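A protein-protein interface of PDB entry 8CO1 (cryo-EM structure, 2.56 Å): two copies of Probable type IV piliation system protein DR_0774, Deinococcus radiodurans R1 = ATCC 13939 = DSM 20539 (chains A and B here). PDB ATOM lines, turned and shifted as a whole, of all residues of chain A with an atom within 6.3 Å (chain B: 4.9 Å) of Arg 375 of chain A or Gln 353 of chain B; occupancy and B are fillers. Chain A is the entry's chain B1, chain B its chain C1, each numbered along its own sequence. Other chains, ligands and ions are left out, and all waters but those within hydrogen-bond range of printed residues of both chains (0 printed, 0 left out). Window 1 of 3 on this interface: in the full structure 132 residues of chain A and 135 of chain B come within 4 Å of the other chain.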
ATOM      1  N   ARG A 326     -14.613  10.647  17.284  1.00  0.00           N
ATOM      2  CA  ARG A 326     -14.122  11.979  17.627  1.00  0.00           C
ATOM      3  C   ARG A 326     -15.333  12.842  17.928  1.00  0.00           C
ATOM      4  O   ARG A 326     -16.171  13.069  17.054  1.00  0.00           O
ATOM      5  CB  ARG A 326     -13.309  12.571  16.488  1.00  0.00           C
ATOM      6  CG  ARG A 326     -12.355  11.601  15.897  1.00  0.00           C
ATOM      7  CD  ARG A 326     -12.378  11.716  14.414  1.00  0.00           C
ATOM      8  NE  ARG A 326     -11.918  13.024  13.988  1.00  0.00           N
ATOM      9  CZ  ARG A 326     -12.119  13.514  12.775  1.00  0.00           C
ATOM     10  NH1 ARG A 326     -12.785  12.803  11.877  1.00  0.00           N
ATOM     11  NH2 ARG A 326     -11.663  14.716  12.462  1.00  0.00           N
ATOM     12  N   GLY A 327     -15.428  13.323  19.154  1.00  0.00           N
ATOM     13  CA  GLY A 327     -16.631  14.004  19.570  1.00  0.00           C
ATOM     14  C   GLY A 327     -17.317  13.167  20.616  1.00  0.00           C
ATOM     15  O   GLY A 327     -16.672  12.330  21.245  1.00  0.00           O
ATOM     16  N   GLN A 328     -18.608  13.361  20.822  1.00  0.00           N
ATOM     17  CA  GLN A 328     -19.310  12.502  21.753  1.00  0.00           C
ATOM     18  C   GLN A 328     -19.464  11.123  21.141  1.00  0.00           C
ATOM     19  O   GLN A 328     -19.404  10.959  19.925  1.00  0.00           O
ATOM     20  CB  GLN A 328     -20.677  13.076  22.102  1.00  0.00           C
ATOM     21  CG  GLN A 328     -20.628  14.461  22.710  1.00  0.00           C
ATOM     22  CD  GLN A 328     -19.855  14.493  24.007  1.00  0.00           C
ATOM     23  OE1 GLN A 328     -18.867  15.212  24.136  1.00  0.00           O
ATOM     24  NE2 GLN A 328     -20.297  13.702  24.974  1.00  0.00           N
ATOM     25  N   LEU A 370     -19.931   9.231   8.542  1.00  0.00           N
ATOM     26  CA  LEU A 370     -19.234   9.601   9.763  1.00  0.00           C
ATOM     27  C   LEU A 370     -18.022  10.456   9.471  1.00  0.00           C
ATOM     28  O   LEU A 370     -17.592  11.230  10.322  1.00  0.00           O
ATOM     29  CB  LEU A 370     -18.823   8.357  10.530  1.00  0.00           C
ATOM     30  CG  LEU A 370     -20.003   7.644  11.150  1.00  0.00           C
ATOM     31  CD1 LEU A 370     -19.547   6.516  12.007  1.00  0.00           C
ATOM     32  CD2 LEU A 370     -20.783   8.631  11.944  1.00  0.00           C
ATOM     33  N   GLU A 371     -17.453  10.336   8.286  1.00  0.00           N
ATOM     34  CA  GLU A 371     -16.368  11.237   7.934  1.00  0.00           C
ATOM     35  C   GLU A 371     -16.862  12.669   7.799  1.00  0.00           C
ATOM     36  O   GLU A 371     -16.072  13.608   7.929  1.00  0.00           O
ATOM     37  CB  GLU A 371     -15.698  10.744   6.656  1.00  0.00           C
ATOM     38  CG  GLU A 371     -14.422  11.441   6.290  1.00  0.00           C
ATOM     39  CD  GLU A 371     -14.682  12.719   5.544  1.00  0.00           C
ATOM     40  OE1 GLU A 371     -15.722  12.793   4.856  1.00  0.00           O
ATOM     41  OE2 GLU A 371     -13.859  13.653   5.644  1.00  0.00           O
ATOM     42  N   GLN A 372     -18.164  12.862   7.591  1.00  0.00           N
ATOM     43  CA  GLN A 372     -18.700  14.194   7.332  1.00  0.00           C
ATOM     44  C   GLN A 372     -19.246  14.845   8.596  1.00  0.00           C
ATOM     45  O   GLN A 372     -18.940  16.002   8.888  1.00  0.00           O
ATOM     46  CB  GLN A 372     -19.793  14.113   6.270  1.00  0.00           C
ATOM     47  CG  GLN A 372     -19.288  14.222   4.861  1.00  0.00           C
ATOM     48  CD  GLN A 372     -20.368  13.954   3.847  1.00  0.00           C
ATOM     49  OE1 GLN A 372     -21.516  13.716   4.196  1.00  0.00           O
ATOM     50  NE2 GLN A 372     -20.001  13.973   2.578  1.00  0.00           N
ATOM     51  N   VAL A 373     -20.061  14.128   9.354  1.00  0.00           N
ATOM     52  CA  VAL A 373     -20.812  14.731  10.439  1.00  0.00           C
ATOM     53  C   VAL A 373     -20.145  14.498  11.791  1.00  0.00           C
ATOM     54  O   VAL A 373     -20.805  14.583  12.819  1.00  0.00           O
ATOM     55  CB  VAL A 373     -22.259  14.236  10.470  1.00  0.00           C
ATOM     56  CG1 VAL A 373     -22.956  14.579   9.195  1.00  0.00           C
ATOM     57  CG2 VAL A 373     -22.293  12.762  10.717  1.00  0.00           C
ATOM     58  N   ASP A 374     -18.852  14.205  11.813  1.00  0.00           N
ATOM     59  CA  ASP A 374     -18.176  13.858  13.058  1.00  0.00           C
ATOM     60  C   ASP A 374     -16.862  14.613  13.140  1.00  0.00           C
ATOM     61  O   ASP A 374     -15.908  14.279  12.433  1.00  0.00           O
ATOM     62  CB  ASP A 374     -17.943  12.360  13.137  1.00  0.00           C
ATOM     63  CG  ASP A 374     -17.547  11.918  14.494  1.00  0.00           C
ATOM     64  OD1 ASP A 374     -18.350  12.106  15.422  1.00  0.00           O
ATOM     65  OD2 ASP A 374     -16.441  11.372  14.633  1.00  0.00           O
ATOM     66  N   ARG A 375     -16.812  15.617  14.000  1.00  0.00           N
ATOM     67  CA  ARG A 375     -15.624  16.428  14.202  1.00  0.00           C
ATOM     68  C   ARG A 375     -15.486  16.727  15.685  1.00  0.00           C
ATOM     69  O   ARG A 375     -16.471  16.676  16.426  1.00  0.00           O
ATOM     70  CB  ARG A 375     -15.693  17.734  13.406  1.00  0.00           C
ATOM     71  CG  ARG A 375     -15.646  17.554  11.913  1.00  0.00           C
ATOM     72  CD  ARG A 375     -16.124  18.818  11.253  1.00  0.00           C
ATOM     73  NE  ARG A 375     -17.330  19.295  11.913  1.00  0.00           N
ATOM     74  CZ  ARG A 375     -18.550  19.156  11.416  1.00  0.00           C
ATOM     75  NH1 ARG A 375     -18.724  18.563  10.246  1.00  0.00           N
ATOM     76  NH2 ARG A 375     -19.595  19.612  12.087  1.00  0.00           N
ATOM     77  N   PRO A 376     -14.277  17.040  16.147  1.00  0.00           N
ATOM     78  CA  PRO A 376     -14.085  17.289  17.577  1.00  0.00           C
ATOM     79  C   PRO A 376     -14.890  18.485  18.050  1.00  0.00           C
ATOM     80  O   PRO A 376     -15.157  19.422  17.299  1.00  0.00           O
ATOM     81  CB  PRO A 376     -12.582  17.550  17.692  1.00  0.00           C
ATOM     82  CG  PRO A 376     -11.995  16.980  16.464  1.00  0.00           C
ATOM     83  CD  PRO A 376     -13.012  17.137  15.404  1.00  0.00           C
ATOM     84  N   ALA A 377     -15.278  18.444  19.319  1.00  0.00           N
ATOM     85  CA  ALA A 377     -16.103  19.492  19.888  1.00  0.00           C
ATOM     86  C   ALA A 377     -15.327  20.805  19.966  1.00  0.00           C
ATOM     87  O   ALA A 377     -14.097  20.811  19.944  1.00  0.00           O
ATOM     88  CB  ALA A 377     -16.583  19.084  21.277  1.00  0.00           C
ATOM     89  N   ILE B 322     -26.996  16.945   4.184  1.00  0.00           N
ATOM     90  CA  ILE B 322     -26.666  17.358   5.540  1.00  0.00           C
ATOM     91  C   ILE B 322     -26.888  18.855   5.638  1.00  0.00           C
ATOM     92  O   ILE B 322     -26.349  19.623   4.834  1.00  0.00           O
ATOM     93  CB  ILE B 322     -25.220  16.997   5.893  1.00  0.00           C
ATOM     94  CG1 ILE B 322     -25.113  15.506   6.137  1.00  0.00           C
ATOM     95  CG2 ILE B 322     -24.772  17.735   7.105  1.00  0.00           C
ATOM     96  CD1 ILE B 322     -23.780  14.972   5.825  1.00  0.00           C
ATOM     97  N   TYR B 323     -27.672  19.271   6.618  1.00  0.00           N
ATOM     98  CA  TYR B 323     -27.999  20.671   6.802  1.00  0.00           C
ATOM     99  C   TYR B 323     -27.347  21.167   8.081  1.00  0.00           C
ATOM    100  O   TYR B 323     -27.356  20.472   9.099  1.00  0.00           O
ATOM    101  CB  TYR B 323     -29.509  20.877   6.858  1.00  0.00           C
ATOM    102  CG  TYR B 323     -29.885  22.323   6.905  1.00  0.00           C
ATOM    103  CD1 TYR B 323     -29.641  23.150   5.827  1.00  0.00           C
ATOM    104  CD2 TYR B 323     -30.456  22.873   8.032  1.00  0.00           C
ATOM    105  CE1 TYR B 323     -29.965  24.477   5.868  1.00  0.00           C
ATOM    106  CE2 TYR B 323     -30.780  24.200   8.079  1.00  0.00           C
ATOM    107  CZ  TYR B 323     -30.530  24.995   6.996  1.00  0.00           C
ATOM    108  OH  TYR B 323     -30.852  26.322   7.041  1.00  0.00           O
ATOM    109  N   THR B 324     -26.762  22.358   8.016  1.00  0.00           N
ATOM    110  CA  THR B 324     -26.063  22.966   9.145  1.00  0.00           C
ATOM    111  C   THR B 324     -26.932  24.093   9.679  1.00  0.00           C
ATOM    112  O   THR B 324     -26.844  25.229   9.226  1.00  0.00           O
ATOM    113  CB  THR B 324     -24.716  23.499   8.710  1.00  0.00           C
ATOM    114  OG1 THR B 324     -24.929  24.693   7.953  1.00  0.00           O
ATOM    115  CG2 THR B 324     -24.015  22.495   7.836  1.00  0.00           C
ATOM    116  N   VAL B 325     -27.760  23.777  10.672  1.00  0.00           N
ATOM    117  CA  VAL B 325     -28.777  24.719  11.112  1.00  0.00           C
ATOM    118  C   VAL B 325     -28.149  25.970  11.700  1.00  0.00           C
ATOM    119  O   VAL B 325     -27.195  25.908  12.481  1.00  0.00           O
ATOM    120  CB  VAL B 325     -29.720  24.035  12.109  1.00  0.00           C
ATOM    121  CG1 VAL B 325     -28.985  23.656  13.327  1.00  0.00           C
ATOM    122  CG2 VAL B 325     -30.771  24.989  12.507  1.00  0.00           C
ATOM    123  N   THR B 346     -32.806  13.673  10.956  1.00  0.00           N
ATOM    124  CA  THR B 346     -32.083  13.034  12.037  1.00  0.00           C
ATOM    125  C   THR B 346     -30.960  13.932  12.519  1.00  0.00           C
ATOM    126  O   THR B 346     -30.137  14.366  11.705  1.00  0.00           O
ATOM    127  CB  THR B 346     -31.508  11.700  11.574  1.00  0.00           C
ATOM    128  OG1 THR B 346     -32.577  10.807  11.254  1.00  0.00           O
ATOM    129  CG2 THR B 346     -30.673  11.085  12.663  1.00  0.00           C
ATOM    130  N   PRO B 347     -30.886  14.233  13.810  1.00  0.00           N
ATOM    131  CA  PRO B 347     -29.848  15.130  14.310  1.00  0.00           C
ATOM    132  C   PRO B 347     -28.564  14.392  14.631  1.00  0.00           C
ATOM    133  O   PRO B 347     -28.571  13.260  15.111  1.00  0.00           O
ATOM    134  CB  PRO B 347     -30.468  15.687  15.599  1.00  0.00           C
ATOM    135  CG  PRO B 347     -31.869  15.144  15.649  1.00  0.00           C
ATOM    136  CD  PRO B 347     -31.840  13.894  14.865  1.00  0.00           C
ATOM    137  N   VAL B 348     -27.446  15.059  14.370  1.00  0.00           N
ATOM    138  CA  VAL B 348     -26.132  14.548  14.786  1.00  0.00           C
ATOM    139  C   VAL B 348     -25.882  15.118  16.175  1.00  0.00           C
ATOM    140  O   VAL B 348     -25.162  16.096  16.369  1.00  0.00           O
ATOM    141  CB  VAL B 348     -25.032  14.920  13.800  1.00  0.00           C
ATOM    142  CG1 VAL B 348     -23.754  14.229  14.172  1.00  0.00           C
ATOM    143  CG2 VAL B 348     -25.441  14.545  12.414  1.00  0.00           C
ATOM    144  N   THR B 351     -25.086  19.236  17.811  1.00  0.00           N
ATOM    145  CA  THR B 351     -23.953  19.865  17.153  1.00  0.00           C
ATOM    146  C   THR B 351     -24.395  20.831  16.071  1.00  0.00           C
ATOM    147  O   THR B 351     -23.572  21.235  15.247  1.00  0.00           O
ATOM    148  CB  THR B 351     -23.020  18.823  16.547  1.00  0.00           C
ATOM    149  OG1 THR B 351     -23.771  17.963  15.689  1.00  0.00           O
ATOM    150  CG2 THR B 351     -22.378  18.000  17.631  1.00  0.00           C
ATOM    151  N   GLY B 352     -25.669  21.203  16.050  1.00  0.00           N
ATOM    152  CA  GLY B 352     -26.150  22.116  15.044  1.00  0.00           C
ATOM    153  C   GLY B 352     -26.118  21.566  13.646  1.00  0.00           C
ATOM    154  O   GLY B 352     -26.188  22.339  12.689  1.00  0.00           O
ATOM    155  N   GLN B 353     -25.999  20.257  13.495  1.00  0.00           N
ATOM    156  CA  GLN B 353     -26.073  19.606  12.202  1.00  0.00           C
ATOM    157  C   GLN B 353     -27.309  18.736  12.170  1.00  0.00           C
ATOM    158  O   GLN B 353     -27.898  18.430  13.207  1.00  0.00           O
ATOM    159  CB  GLN B 353     -24.833  18.774  11.919  1.00  0.00           C
ATOM    160  CG  GLN B 353     -23.786  19.553  11.202  1.00  0.00           C
ATOM    161  CD  GLN B 353     -22.560  18.750  10.962  1.00  0.00           C
ATOM    162  OE1 GLN B 353     -21.728  19.099  10.135  1.00  0.00           O
ATOM    163  NE2 GLN B 353     -22.410  17.682  11.717  1.00  0.00           N
ATOM    164  N   LEU B 354     -27.711  18.359  10.970  1.00  0.00           N
ATOM    165  CA  LEU B 354     -29.042  17.806  10.795  1.00  0.00           C
ATOM    166  C   LEU B 354     -29.011  16.991   9.516  1.00  0.00           C
ATOM    167  O   LEU B 354     -28.927  17.565   8.430  1.00  0.00           O
ATOM    168  CB  LEU B 354     -30.051  18.938  10.722  1.00  0.00           C
ATOM    169  CG  LEU B 354     -31.527  18.771  10.993  1.00  0.00           C
ATOM    170  CD1 LEU B 354     -31.699  18.470  12.443  1.00  0.00           C
ATOM    171  CD2 LEU B 354     -32.199  20.055  10.664  1.00  0.00           C
ATOM    172  N   VAL B 355     -29.038  15.670   9.640  1.00  0.00           N
ATOM    173  CA  VAL B 355     -28.986  14.771   8.495  1.00  0.00           C
ATOM    174  C   VAL B 355     -30.414  14.439   8.113  1.00  0.00           C
ATOM    175  O   VAL B 355     -31.100  13.714   8.840  1.00  0.00           O
ATOM    176  CB  VAL B 355     -28.197  13.495   8.810  1.00  0.00           C
ATOM    177  CG1 VAL B 355     -28.323  12.545   7.668  1.00  0.00           C
ATOM    178  CG2 VAL B 355     -26.755  13.817   9.035  1.00  0.00           C
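O of Thr 346 of chain B lies within hydrogen-bond range of N of Val 355 of chain B (2.7 Å).
NH1 of Arg 375 of chain A lies within hydrogen-bond range of O of Gln 372 of chain A, at 2.9 Å.
The backbone carbonyl oxygen of Val 348 of chain B sits at hydrogen-bond distance from the side-chain hydroxyl of Thr 351 of chain B (2.4 Å).
Among the printed residues, merely in contact across the chains: Gln 372 of chain A with Ile 322 of chain B, Val 373 of chain A with Ile 322 of chain B, Val 373 of chain A with Val 348 of chain B, Val 373 of chain A with Gln 353 of chain B and Val 373 of chain A with Val 355 of chain B.
Arg 375 of chain A touches one residue of chain B.
Gln 353 of chain B touches two residues of chain A.
Printed residues of chain A within 4 Å of Val 355 of chain B: Val 373 (3.9 Å).
Printed residues of chain A within 4 Å of Val 348 of chain B: Val 373.
Thr 324 of chain B touches none of the printed residues of chain A.
The nearest printed residue of chain B that does not touch Arg 375 of chain A is Thr 351 of chain B (5.3 Å).
Hydrophobic or aromatic side chains of chain B that line the printed part of chain A: Ile 322, Val 348 and Val 355.
Of the 11 printed residues of chain A, 3 touch a printed residue of chain B.
Among the printed residues, 6 pairs touch across the chains.
Among the printed residues, no Asp or Glu carboxylate lies within 4 Å of a Lys or Arg side-chain nitrogen of the other chain.
The side-chain amide oxygen of Gln 353 of chain B sits at hydrogen-bond distance from the guanidinium group of Arg 375 of chain A (2.9 Å).
No position is printed for both chains.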
